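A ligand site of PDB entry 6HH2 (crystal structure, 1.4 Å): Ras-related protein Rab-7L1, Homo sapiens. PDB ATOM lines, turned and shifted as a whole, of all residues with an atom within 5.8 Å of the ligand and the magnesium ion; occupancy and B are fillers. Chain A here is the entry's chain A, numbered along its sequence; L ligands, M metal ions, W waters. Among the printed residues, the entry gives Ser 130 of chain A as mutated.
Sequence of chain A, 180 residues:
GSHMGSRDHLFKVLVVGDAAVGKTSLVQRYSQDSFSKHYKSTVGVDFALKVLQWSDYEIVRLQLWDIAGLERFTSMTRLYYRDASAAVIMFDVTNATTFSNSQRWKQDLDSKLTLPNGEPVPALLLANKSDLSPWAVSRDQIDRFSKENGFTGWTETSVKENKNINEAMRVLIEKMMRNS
The backbone NH (N) of Lys 160 lies within hydrogen-bond range of an oxygen (O11) of the ligand, at 3.3 Å. The side-chain hydroxyl of Ser 158 lies close to an oxygen (O11) of the ligand (3.4 Å). N of Thr 24 lies within hydrogen-bond range of O5 of the ligand (3.5 Å). O4 of the ligand is in hydrogen-bond range of N of Gly 22, at 3.1 Å. The side-chain hydroxyl of Ser 25 sits at hydrogen-bond distance from an oxygen (O5) of the ligand (2.6 Å). The side-chain amino group (NZ) of Lys 23 is in salt-bridge range of an oxygen (O1) of the ligand. ND2 of Asn 128 sits at hydrogen-bond distance from N2 of the ligand, at 3.2 Å. The backbone NH of Lys 23 is in hydrogen-bond range of an oxygen (O1) of the ligand, at 2.9 Å. The backbone NH (N) of Ser 25 is in hydrogen-bond range of an oxygen (O5) of the ligand. The side-chain amino group of Lys 129 is in hydrogen-bond range of an oxygen (O8) of the ligand. The backbone NH (N) of Val 21 lies within hydrogen-bond range of an oxygen (O1) of the ligand. The backbone NH of Val 159 lies within hydrogen-bond range of an oxygen (O11) of the ligand (2.9 Å). A nitrogen (N3) of the ligand is in hydrogen-bond range of the side-chain carboxylate (OD1) of Asp 131 (2.8 Å). The backbone NH (N) of Lys 129 sits close to an oxygen (O11) of the ligand, at 3.4 Å. N of Ala 20 sits at hydrogen-bond distance from O2 of the ligand (2.8 Å).
O of Thr 157 lies within hydrogen-bond range of N of Lys 129, at 3.2 Å. O of Val 21 lies within hydrogen-bond range of ND2 of Asn 128 (2.9 Å). The side-chain amide oxygen of Asn 128 sits at hydrogen-bond distance from the side-chain hydroxyl of Thr 157 (2.8 Å). The side-chain hydroxyl of Ser 158 lies within hydrogen-bond range of the backbone NH of Glu 161 (3.0 Å). The side-chain amino group of Lys 129 is in hydrogen-bond range of the backbone carbonyl oxygen of Ala 20 (3.0 Å). OE1 of Glu 71 lies within salt-bridge range of NZ of Lys 23 (2.7 Å). The side-chain amino group (NZ) of Lys 23 lies within hydrogen-bond range of the backbone carbonyl oxygen (O) of Gly 17, at 3.1 Å. OD1 of Asp 131 lies within hydrogen-bond range of OG of Ser 158 (2.7 Å).
O of Asp 18 touches O1 of the ligand, 3.7 Å away. C of Ala 19 touches O2 of the ligand, 3.8 Å away. OE1 of Glu 71 touches O2 of the ligand, 3.96 Å away. Leu 132 touches the ligand (CD2 to N4, 3.4 Å). Hydrophobic or aromatic side chains that line the ligand: Val 21, Leu 132 and Val 159. 16 residues have an atom within 4 Å of the ligand: Asp 18, Ala 19, Ala 20, Val 21, Gly 22, Lys 23, Thr 24, Ser 25, Glu 71, Asn 128, Lys 129, Asp 131, Leu 132, Ser 158, Val 159 and Lys 160. The nearest printed residue that does not touch the ligand is Thr 157 (4.5 Å).
Glu 71 touches the magnesium ion. Of the 24 residues printed, 2 come within 4 Å of the magnesium ion.
Water W7 is bound to the magnesium ion, 2.0 Å away. The magnesium ion is bound by an oxygen (O3) of the ligand, 2.0 Å away. The side-chain hydroxyl (OG1) of Thr 24 binds the magnesium ion. The magnesium ion is bound by water W10 (2.1 Å). Water W6 is bound to the magnesium ion, at 2.1 Å. Water W2 binds the magnesium ion (2.1 Å). The magnesium ion has six donor atoms within binding distance.
Water W10 lies within hydrogen-bond range of the side-chain carboxylate of Asp 66 and the side-chain carboxylate of Glu 71. Water W2 lies within hydrogen-bond range of O2 of the ligand (2.6 Å) and OE2 of Glu 71 (2.7 Å). Water W3 bridges the side-chain hydroxyl (OG) of Ser 25 (2.7 Å) and an oxygen (O10) of the ligand (2.8 Å). Water W11 bridges a nitrogen (N4) of the ligand (3.0 Å) and the side-chain amino group of Lys 160 (3.5 Å). Water W1 bridges NZ of Lys 129 (2.9 Å) and N5 of the ligand (3.0 Å).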
ATOM      1  N   GLY A  17     -21.822  21.097 -30.655  1.00  0.00           N
ATOM      2  CA  GLY A  17     -20.647  20.343 -31.034  1.00  0.00           C
ATOM      3  C   GLY A  17     -20.760  18.925 -30.525  1.00  0.00           C
ATOM      4  O   GLY A  17     -21.626  18.594 -29.707  1.00  0.00           O
ATOM      5  N   ASP A  18     -19.886  18.073 -31.030  1.00  0.00           N
ATOM      6  CA  ASP A  18     -19.972  16.656 -30.672  1.00  0.00           C
ATOM      7  C   ASP A  18     -19.672  16.428 -29.183  1.00  0.00           C
ATOM      8  O   ASP A  18     -19.126  17.283 -28.469  1.00  0.00           O
ATOM      9  CB  ASP A  18     -18.996  15.857 -31.500  1.00  0.00           C
ATOM     10  CG  ASP A  18     -19.413  15.688 -32.949  1.00  0.00           C
ATOM     11  OD1 ASP A  18     -20.478  16.204 -33.361  1.00  0.00           O
ATOM     12  OD2 ASP A  18     -18.642  15.019 -33.654  1.00  0.00           O
ATOM     13  N   ALA A  19     -20.023  15.249 -28.690  1.00  0.00           N
ATOM     14  CA  ALA A  19     -19.572  14.862 -27.360  1.00  0.00           C
ATOM     15  C   ALA A  19     -18.060  14.985 -27.239  1.00  0.00           C
ATOM     16  O   ALA A  19     -17.302  14.690 -28.177  1.00  0.00           O
ATOM     17  CB  ALA A  19     -20.013  13.414 -27.044  1.00  0.00           C
ATOM     18  N   ALA A  20     -17.631  15.402 -26.046  1.00  0.00           N
ATOM     19  CA  ALA A  20     -16.235  15.376 -25.584  1.00  0.00           C
ATOM     20  C   ALA A  20     -15.365  16.429 -26.238  1.00  0.00           C
ATOM     21  O   ALA A  20     -14.150  16.295 -26.223  1.00  0.00           O
ATOM     22  CB  ALA A  20     -15.563  13.987 -25.696  1.00  0.00           C
ATOM     23  N   VAL A  21     -15.970  17.479 -26.790  1.00  0.00           N
ATOM     24  CA  VAL A  21     -15.169  18.559 -27.357  1.00  0.00           C
ATOM     25  C   VAL A  21     -14.866  19.671 -26.381  1.00  0.00           C
ATOM     26  O   VAL A  21     -14.030  20.536 -26.718  1.00  0.00           O
ATOM     27  CB  VAL A  21     -15.783  19.134 -28.639  1.00  0.00           C
ATOM     28  CG1 VAL A  21     -15.930  17.984 -29.713  1.00  0.00           C
ATOM     29  CG2 VAL A  21     -17.086  19.873 -28.393  1.00  0.00           C
ATOM     30  N   GLY A  22     -15.524  19.723 -25.237  1.00  0.00           N
ATOM     31  CA  GLY A  22     -15.310  20.772 -24.251  1.00  0.00           C
ATOM     32  C   GLY A  22     -16.486  21.722 -23.987  1.00  0.00           C
ATOM     33  O   GLY A  22     -16.265  22.808 -23.431  1.00  0.00           O
ATOM     34  N   LYS A  23     -17.709  21.377 -24.397  1.00  0.00           N
ATOM     35  CA  LYS A  23     -18.811  22.344 -24.296  1.00  0.00           C
ATOM     36  C   LYS A  23     -19.172  22.603 -22.844  1.00  0.00           C
ATOM     37  O   LYS A  23     -19.328  23.763 -22.458  1.00  0.00           O
ATOM     38  CB  LYS A  23     -20.039  21.797 -25.028  1.00  0.00           C
ATOM     39  CG  LYS A  23     -19.761  21.594 -26.513  1.00  0.00           C
ATOM     40  CD  LYS A  23     -21.053  21.131 -27.268  1.00  0.00           C
ATOM     41  CE  LYS A  23     -21.706  19.859 -26.683  1.00  0.00           C
ATOM     42  NZ  LYS A  23     -20.739  18.706 -26.715  1.00  0.00           N
ATOM     43  N   THR A  24     -19.441  21.557 -22.044  1.00  0.00           N
ATOM     44  CA  THR A  24     -19.808  21.787 -20.646  1.00  0.00           C
ATOM     45  C   THR A  24     -18.685  22.502 -19.921  1.00  0.00           C
ATOM     46  O   THR A  24     -18.954  23.394 -19.102  1.00  0.00           O
ATOM     47  CB  THR A  24     -20.208  20.465 -20.014  1.00  0.00           C
ATOM     48  OG1 THR A  24     -21.273  19.892 -20.796  1.00  0.00           O
ATOM     49  CG2 THR A  24     -20.720  20.675 -18.558  1.00  0.00           C
ATOM     50  N   SER A  25     -17.448  22.155 -20.240  1.00  0.00           N
ATOM     51  CA  SER A  25     -16.314  22.828 -19.610  1.00  0.00           C
ATOM     52  C   SER A  25     -16.296  24.324 -19.979  1.00  0.00           C
ATOM     53  O   SER A  25     -16.026  25.165 -19.114  1.00  0.00           O
ATOM     54  CB  SER A  25     -15.006  22.166 -20.044  1.00  0.00           C
ATOM     55  OG  SER A  25     -14.953  20.837 -19.574  1.00  0.00           O
ATOM     56  N   LEU A  26     -16.563  24.573 -21.248  1.00  0.00           N
ATOM     57  CA  LEU A  26     -16.650  26.072 -21.591  1.00  0.00           C
ATOM     58  C   LEU A  26     -17.794  26.888 -20.784  1.00  0.00           C
ATOM     59  O   LEU A  26     -17.616  27.963 -20.165  1.00  0.00           O
ATOM     60  CB  LEU A  26     -16.878  26.246 -23.098  1.00  0.00           C
ATOM     61  CG  LEU A  26     -16.843  27.692 -23.539  1.00  0.00           C
ATOM     62  CD1 LEU A  26     -16.103  27.777 -24.942  1.00  0.00           C
ATOM     63  CD2 LEU A  26     -18.165  28.245 -23.628  1.00  0.00           C
ATOM     64  N   GLN A  28     -19.099  25.983 -17.915  1.00  0.00           N
ATOM     65  CA  GLN A  28     -18.728  26.081 -16.503  1.00  0.00           C
ATOM     66  C   GLN A  28     -17.696  27.153 -16.266  1.00  0.00           C
ATOM     67  O   GLN A  28     -17.737  27.834 -15.238  1.00  0.00           O
ATOM     68  CB  GLN A  28     -18.195  24.736 -16.029  1.00  0.00           C
ATOM     69  CG  GLN A  28     -19.292  23.683 -15.957  1.00  0.00           C
ATOM     70  CD  GLN A  28     -18.753  22.286 -15.680  1.00  0.00           C
ATOM     71  OE1 GLN A  28     -17.618  21.947 -16.027  1.00  0.00           O
ATOM     72  NE2 GLN A  28     -19.573  21.473 -15.035  1.00  0.00           N
ATOM     73  N   ASP A  66     -26.201  24.595 -23.355  1.00  0.00           N
ATOM     74  CA  ASP A  66     -25.353  23.451 -23.748  1.00  0.00           C
ATOM     75  C   ASP A  66     -26.270  22.344 -24.316  1.00  0.00           C
ATOM     76  O   ASP A  66     -27.206  21.882 -23.642  1.00  0.00           O
ATOM     77  CB  ASP A  66     -24.695  22.979 -22.448  1.00  0.00           C
ATOM     78  CG  ASP A  66     -23.739  21.824 -22.571  1.00  0.00           C
ATOM     79  OD1 ASP A  66     -23.659  21.113 -23.577  1.00  0.00           O
ATOM     80  OD2 ASP A  66     -23.061  21.631 -21.536  1.00  0.00           O
ATOM     81  N   ALA A  68     -25.767  19.322 -24.638  1.00  0.00           N
ATOM     82  CA  ALA A  68     -25.751  18.301 -23.564  1.00  0.00           C
ATOM     83  C   ALA A  68     -26.314  16.954 -23.978  1.00  0.00           C
ATOM     84  O   ALA A  68     -25.759  16.296 -24.872  1.00  0.00           O
ATOM     85  CB  ALA A  68     -26.369  18.873 -22.303  1.00  0.00           C
ATOM     86  N   GLU A  71     -26.379  15.794 -27.697  1.00  0.00           N
ATOM     87  CA  GLU A  71     -25.240  16.195 -28.513  1.00  0.00           C
ATOM     88  C   GLU A  71     -24.844  15.145 -29.530  1.00  0.00           C
ATOM     89  O   GLU A  71     -24.312  15.505 -30.597  1.00  0.00           O
ATOM     90  CB  GLU A  71     -24.051  16.578 -27.616  1.00  0.00           C
ATOM     91  CG  GLU A  71     -23.544  15.423 -26.739  1.00  0.00           C
ATOM     92  CD  GLU A  71     -22.927  15.893 -25.442  1.00  0.00           C
ATOM     93  OE1 GLU A  71     -22.409  17.053 -25.380  1.00  0.00           O
ATOM     94  OE2 GLU A  71     -22.852  15.105 -24.481  1.00  0.00           O
ATOM     95  N   ASN A 128     -11.099  23.739 -30.301  1.00  0.00           N
ATOM     96  CA  ASN A 128     -10.764  23.599 -28.883  1.00  0.00           C
ATOM     97  C   ASN A 128      -9.739  22.488 -28.662  1.00  0.00           C
ATOM     98  O   ASN A 128      -9.476  21.676 -29.544  1.00  0.00           O
ATOM     99  CB  ASN A 128     -12.037  23.379 -28.021  1.00  0.00           C
ATOM    100  CG  ASN A 128     -11.758  23.538 -26.537  1.00  0.00           C
ATOM    101  OD1 ASN A 128     -11.079  24.478 -26.138  1.00  0.00           O
ATOM    102  ND2 ASN A 128     -12.263  22.609 -25.711  1.00  0.00           N
ATOM    103  N   LYS A 129      -9.185  22.457 -27.442  1.00  0.00           N
ATOM    104  CA  LYS A 129      -8.095  21.558 -27.037  1.00  0.00           C
ATOM    105  C   LYS A 129      -6.804  21.866 -27.799  1.00  0.00           C
ATOM    106  O   LYS A 129      -6.007  20.956 -28.089  1.00  0.00           O
ATOM    107  CB  LYS A 129      -8.455  20.057 -27.127  1.00  0.00           C
ATOM    108  CG  LYS A 129      -9.831  19.689 -26.514  1.00  0.00           C
ATOM    109  CD  LYS A 129      -9.836  18.233 -26.116  1.00  0.00           C
ATOM    110  CE  LYS A 129     -11.256  17.902 -25.684  1.00  0.00           C
ATOM    111  NZ  LYS A 129     -11.295  16.432 -25.214  1.00  0.00           N
ATOM    112  N   SER A 130      -6.590  23.150 -28.152  1.00  0.00           N
ATOM    113  CA  SER A 130      -5.407  23.566 -28.884  1.00  0.00           C
ATOM    114  C   SER A 130      -4.116  23.241 -28.160  1.00  0.00           C
ATOM    115  O   SER A 130      -3.068  23.179 -28.797  1.00  0.00           O
ATOM    116  CB  SER A 130      -5.474  25.080 -29.150  1.00  0.00           C
ATOM    117  OG  SER A 130      -5.325  25.801 -27.910  1.00  0.00           O
ATOM    118  N   ASP A 131      -4.190  23.039 -26.829  1.00  0.00           N
ATOM    119  CA  ASP A 131      -3.034  22.675 -26.011  1.00  0.00           C
ATOM    120  C   ASP A 131      -2.529  21.264 -26.280  1.00  0.00           C
ATOM    121  O   ASP A 131      -1.412  20.937 -25.874  1.00  0.00           O
ATOM    122  CB  ASP A 131      -3.422  22.764 -24.521  1.00  0.00           C
ATOM    123  CG  ASP A 131      -4.641  21.918 -24.172  1.00  0.00           C
ATOM    124  OD1 ASP A 131      -5.756  22.340 -24.519  1.00  0.00           O
ATOM    125  OD2 ASP A 131      -4.428  20.875 -23.488  1.00  0.00           O
ATOM    126  N   LEU A 132      -3.341  20.407 -26.900  1.00  0.00           N
ATOM    127  CA  LEU A 132      -2.920  19.051 -27.202  1.00  0.00           C
ATOM    128  C   LEU A 132      -2.125  18.967 -28.494  1.00  0.00           C
ATOM    129  O   LEU A 132      -2.152  19.870 -29.326  1.00  0.00           O
ATOM    130  CB  LEU A 132      -4.127  18.100 -27.254  1.00  0.00           C
ATOM    131  CG  LEU A 132      -4.911  18.019 -25.951  1.00  0.00           C
ATOM    132  CD1 LEU A 132      -6.112  17.091 -26.168  1.00  0.00           C
ATOM    133  CD2 LEU A 132      -4.042  17.554 -24.800  1.00  0.00           C
ATOM    134  N   THR A 157      -8.835  27.594 -29.247  1.00  0.00           N
ATOM    135  CA  THR A 157      -9.053  27.870 -27.832  1.00  0.00           C
ATOM    136  C   THR A 157      -8.562  26.671 -27.035  1.00  0.00           C
ATOM    137  O   THR A 157      -8.375  25.571 -27.577  1.00  0.00           O
ATOM    138  CB  THR A 157     -10.545  27.993 -27.488  1.00  0.00           C
ATOM    139  OG1 THR A 157     -11.245  26.767 -27.818  1.00  0.00           O
ATOM    140  CG2 THR A 157     -11.183  29.132 -28.267  1.00  0.00           C
ATOM    141  N   SER A 158      -8.215  26.929 -25.776  1.00  0.00           N
ATOM    142  CA  SER A 158      -8.034  25.864 -24.800  1.00  0.00           C
ATOM    143  C   SER A 158      -8.893  26.194 -23.604  1.00  0.00           C
ATOM    144  O   SER A 158      -8.539  27.070 -22.803  1.00  0.00           O
ATOM    145  CB  SER A 158      -6.555  25.669 -24.443  1.00  0.00           C
ATOM    146  OG  SER A 158      -6.428  24.708 -23.381  1.00  0.00           O
ATOM    147  N   VAL A 159     -10.023  25.461 -23.403  1.00  0.00           N
ATOM    148  CA  VAL A 159     -10.779  25.693 -22.187  1.00  0.00           C
ATOM    149  C   VAL A 159      -9.936  25.300 -20.989  1.00  0.00           C
ATOM    150  O   VAL A 159      -9.935  25.972 -19.943  1.00  0.00           O
ATOM    151  CB  VAL A 159     -12.093  24.853 -22.232  1.00  0.00           C
ATOM    152  CG1 VAL A 159     -12.846  25.020 -20.915  1.00  0.00           C
ATOM    153  CG2 VAL A 159     -12.976  25.351 -23.389  1.00  0.00           C
ATOM    154  N   LYS A 160      -9.140  24.228 -21.141  1.00  0.00           N
ATOM    155  CA  LYS A 160      -8.301  23.735 -20.051  1.00  0.00           C
ATOM    156  C   LYS A 160      -7.322  24.788 -19.551  1.00  0.00           C
ATOM    157  O   LYS A 160      -7.168  24.969 -18.336  1.00  0.00           O
ATOM    158  CB  LYS A 160      -7.554  22.488 -20.495  1.00  0.00           C
ATOM    159  CG  LYS A 160      -6.520  21.998 -19.489  1.00  0.00           C
ATOM    160  CD  LYS A 160      -5.954  20.641 -19.875  1.00  0.00           C
ATOM    161  CE  LYS A 160      -4.691  20.329 -19.098  1.00  0.00           C
ATOM    162  NZ  LYS A 160      -4.031  19.077 -19.610  1.00  0.00           N
ATOM    163  N   GLU A 161      -6.646  25.484 -20.467  1.00  0.00           N
ATOM    164  CA  GLU A 161      -5.663  26.504 -20.084  1.00  0.00           C
ATOM    165  C   GLU A 161      -6.251  27.906 -20.094  1.00  0.00           C
ATOM    166  O   GLU A 161      -5.507  28.884 -19.914  1.00  0.00           O
ATOM    167  CB  GLU A 161      -4.497  26.485 -21.075  1.00  0.00           C
ATOM    168  CG  GLU A 161      -3.733  25.183 -21.161  1.00  0.00           C
ATOM    169  CD  GLU A 161      -2.609  25.264 -22.193  1.00  0.00           C
ATOM    170  OE1 GLU A 161      -2.665  26.136 -23.127  1.00  0.00           O
ATOM    171  OE2 GLU A 161      -1.630  24.480 -22.052  1.00  0.00           O
HETATM  172  P1  LIG L   1     -18.555  17.950 -23.713  1.00  0.00           P
HETATM  173  O1  LIG L   1     -18.470  18.624 -25.035  1.00  0.00           O
HETATM  174  O2  LIG L   1     -18.826  16.493 -23.797  1.00  0.00           O
HETATM  175  O3  LIG L   1     -19.454  18.668 -22.729  1.00  0.00           O
HETATM  176  O4  LIG L   1     -17.018  18.032 -23.145  1.00  0.00           O
HETATM  177  P2  LIG L   1     -16.527  18.260 -21.639  1.00  0.00           P
HETATM  178  O5  LIG L   1     -16.589  19.711 -21.251  1.00  0.00           O
HETATM  179  O6  LIG L   1     -17.238  17.255 -20.740  1.00  0.00           O
HETATM  180  O7  LIG L   1     -14.981  17.861 -21.751  1.00  0.00           O
HETATM  181  C1  LIG L   1     -14.573  16.557 -22.106  1.00  0.00           C
HETATM  182  C2  LIG L   1     -13.156  16.308 -21.599  1.00  0.00           C
HETATM  183  O8  LIG L   1     -12.249  17.198 -22.321  1.00  0.00           O
HETATM  184  C3  LIG L   1     -13.038  16.714 -20.146  1.00  0.00           C
HETATM  185  O9  LIG L   1     -12.118  15.781 -19.559  1.00  0.00           O
HETATM  186  C4  LIG L   1     -12.429  18.100 -20.189  1.00  0.00           C
HETATM  187  O10 LIG L   1     -11.649  18.339 -19.023  1.00  0.00           O
HETATM  188  C5  LIG L   1     -11.541  17.959 -21.398  1.00  0.00           C
HETATM  189  N1  LIG L   1     -11.277  19.257 -22.034  1.00  0.00           N
HETATM  190  C6  LIG L   1     -12.197  20.236 -22.288  1.00  0.00           C
HETATM  191  N2  LIG L   1     -11.597  21.298 -22.924  1.00  0.00           N
HETATM  192  C7  LIG L   1     -10.288  20.957 -23.066  1.00  0.00           C
HETATM  193  C8  LIG L   1      -9.106  21.613 -23.622  1.00  0.00           C
HETATM  194  O11 LIG L   1      -9.163  22.753 -24.104  1.00  0.00           O
HETATM  195  N3  LIG L   1      -7.971  20.901 -23.587  1.00  0.00           N
HETATM  196  C9  LIG L   1      -7.809  19.686 -23.049  1.00  0.00           C
HETATM  197  N4  LIG L   1      -6.568  19.063 -23.022  1.00  0.00           N
HETATM  198  N5  LIG L   1      -8.867  19.054 -22.477  1.00  0.00           N
HETATM  199  C10 LIG L   1     -10.073  19.658 -22.493  1.00  0.00           C
HETATM  200 MG    MG M   1     -21.116  18.040 -21.731  1.00  0.00          MG
HETATM  201  O   HOH W   1      -9.188  16.205 -23.199  1.00  0.00           O
HETATM  202  O   HOH W   2     -21.174  16.133 -22.691  1.00  0.00           O
HETATM  203  O   HOH W   3     -13.192  20.243 -17.575  1.00  0.00           O
HETATM  204  O   HOH W   4     -10.923  21.495 -18.990  1.00  0.00           O
HETATM  205  O   HOH W   5     -16.915  15.024 -19.643  1.00  0.00           O
HETATM  206  O   HOH W   6     -22.771  17.389 -20.612  1.00  0.00           O
HETATM  207  O   HOH W   7     -19.915  17.288 -20.283  1.00  0.00           O
HETATM  208  O   HOH W   8     -17.914  14.234 -22.533  1.00  0.00           O
HETATM  209  O   HOH W   9     -15.206  13.209 -22.323  1.00  0.00           O
HETATM  210  O   HOH W  10     -22.355  18.751 -23.256  1.00  0.00           O
HETATM  211  O   HOH W  11      -5.934  16.739 -21.311  1.00  0.00           O
HETATM  212  O   HOH W  12     -16.903  18.417 -17.930  1.00  0.00           O
HETATM  213  O   HOH W  13     -12.310  13.935 -23.872  1.00  0.00           O
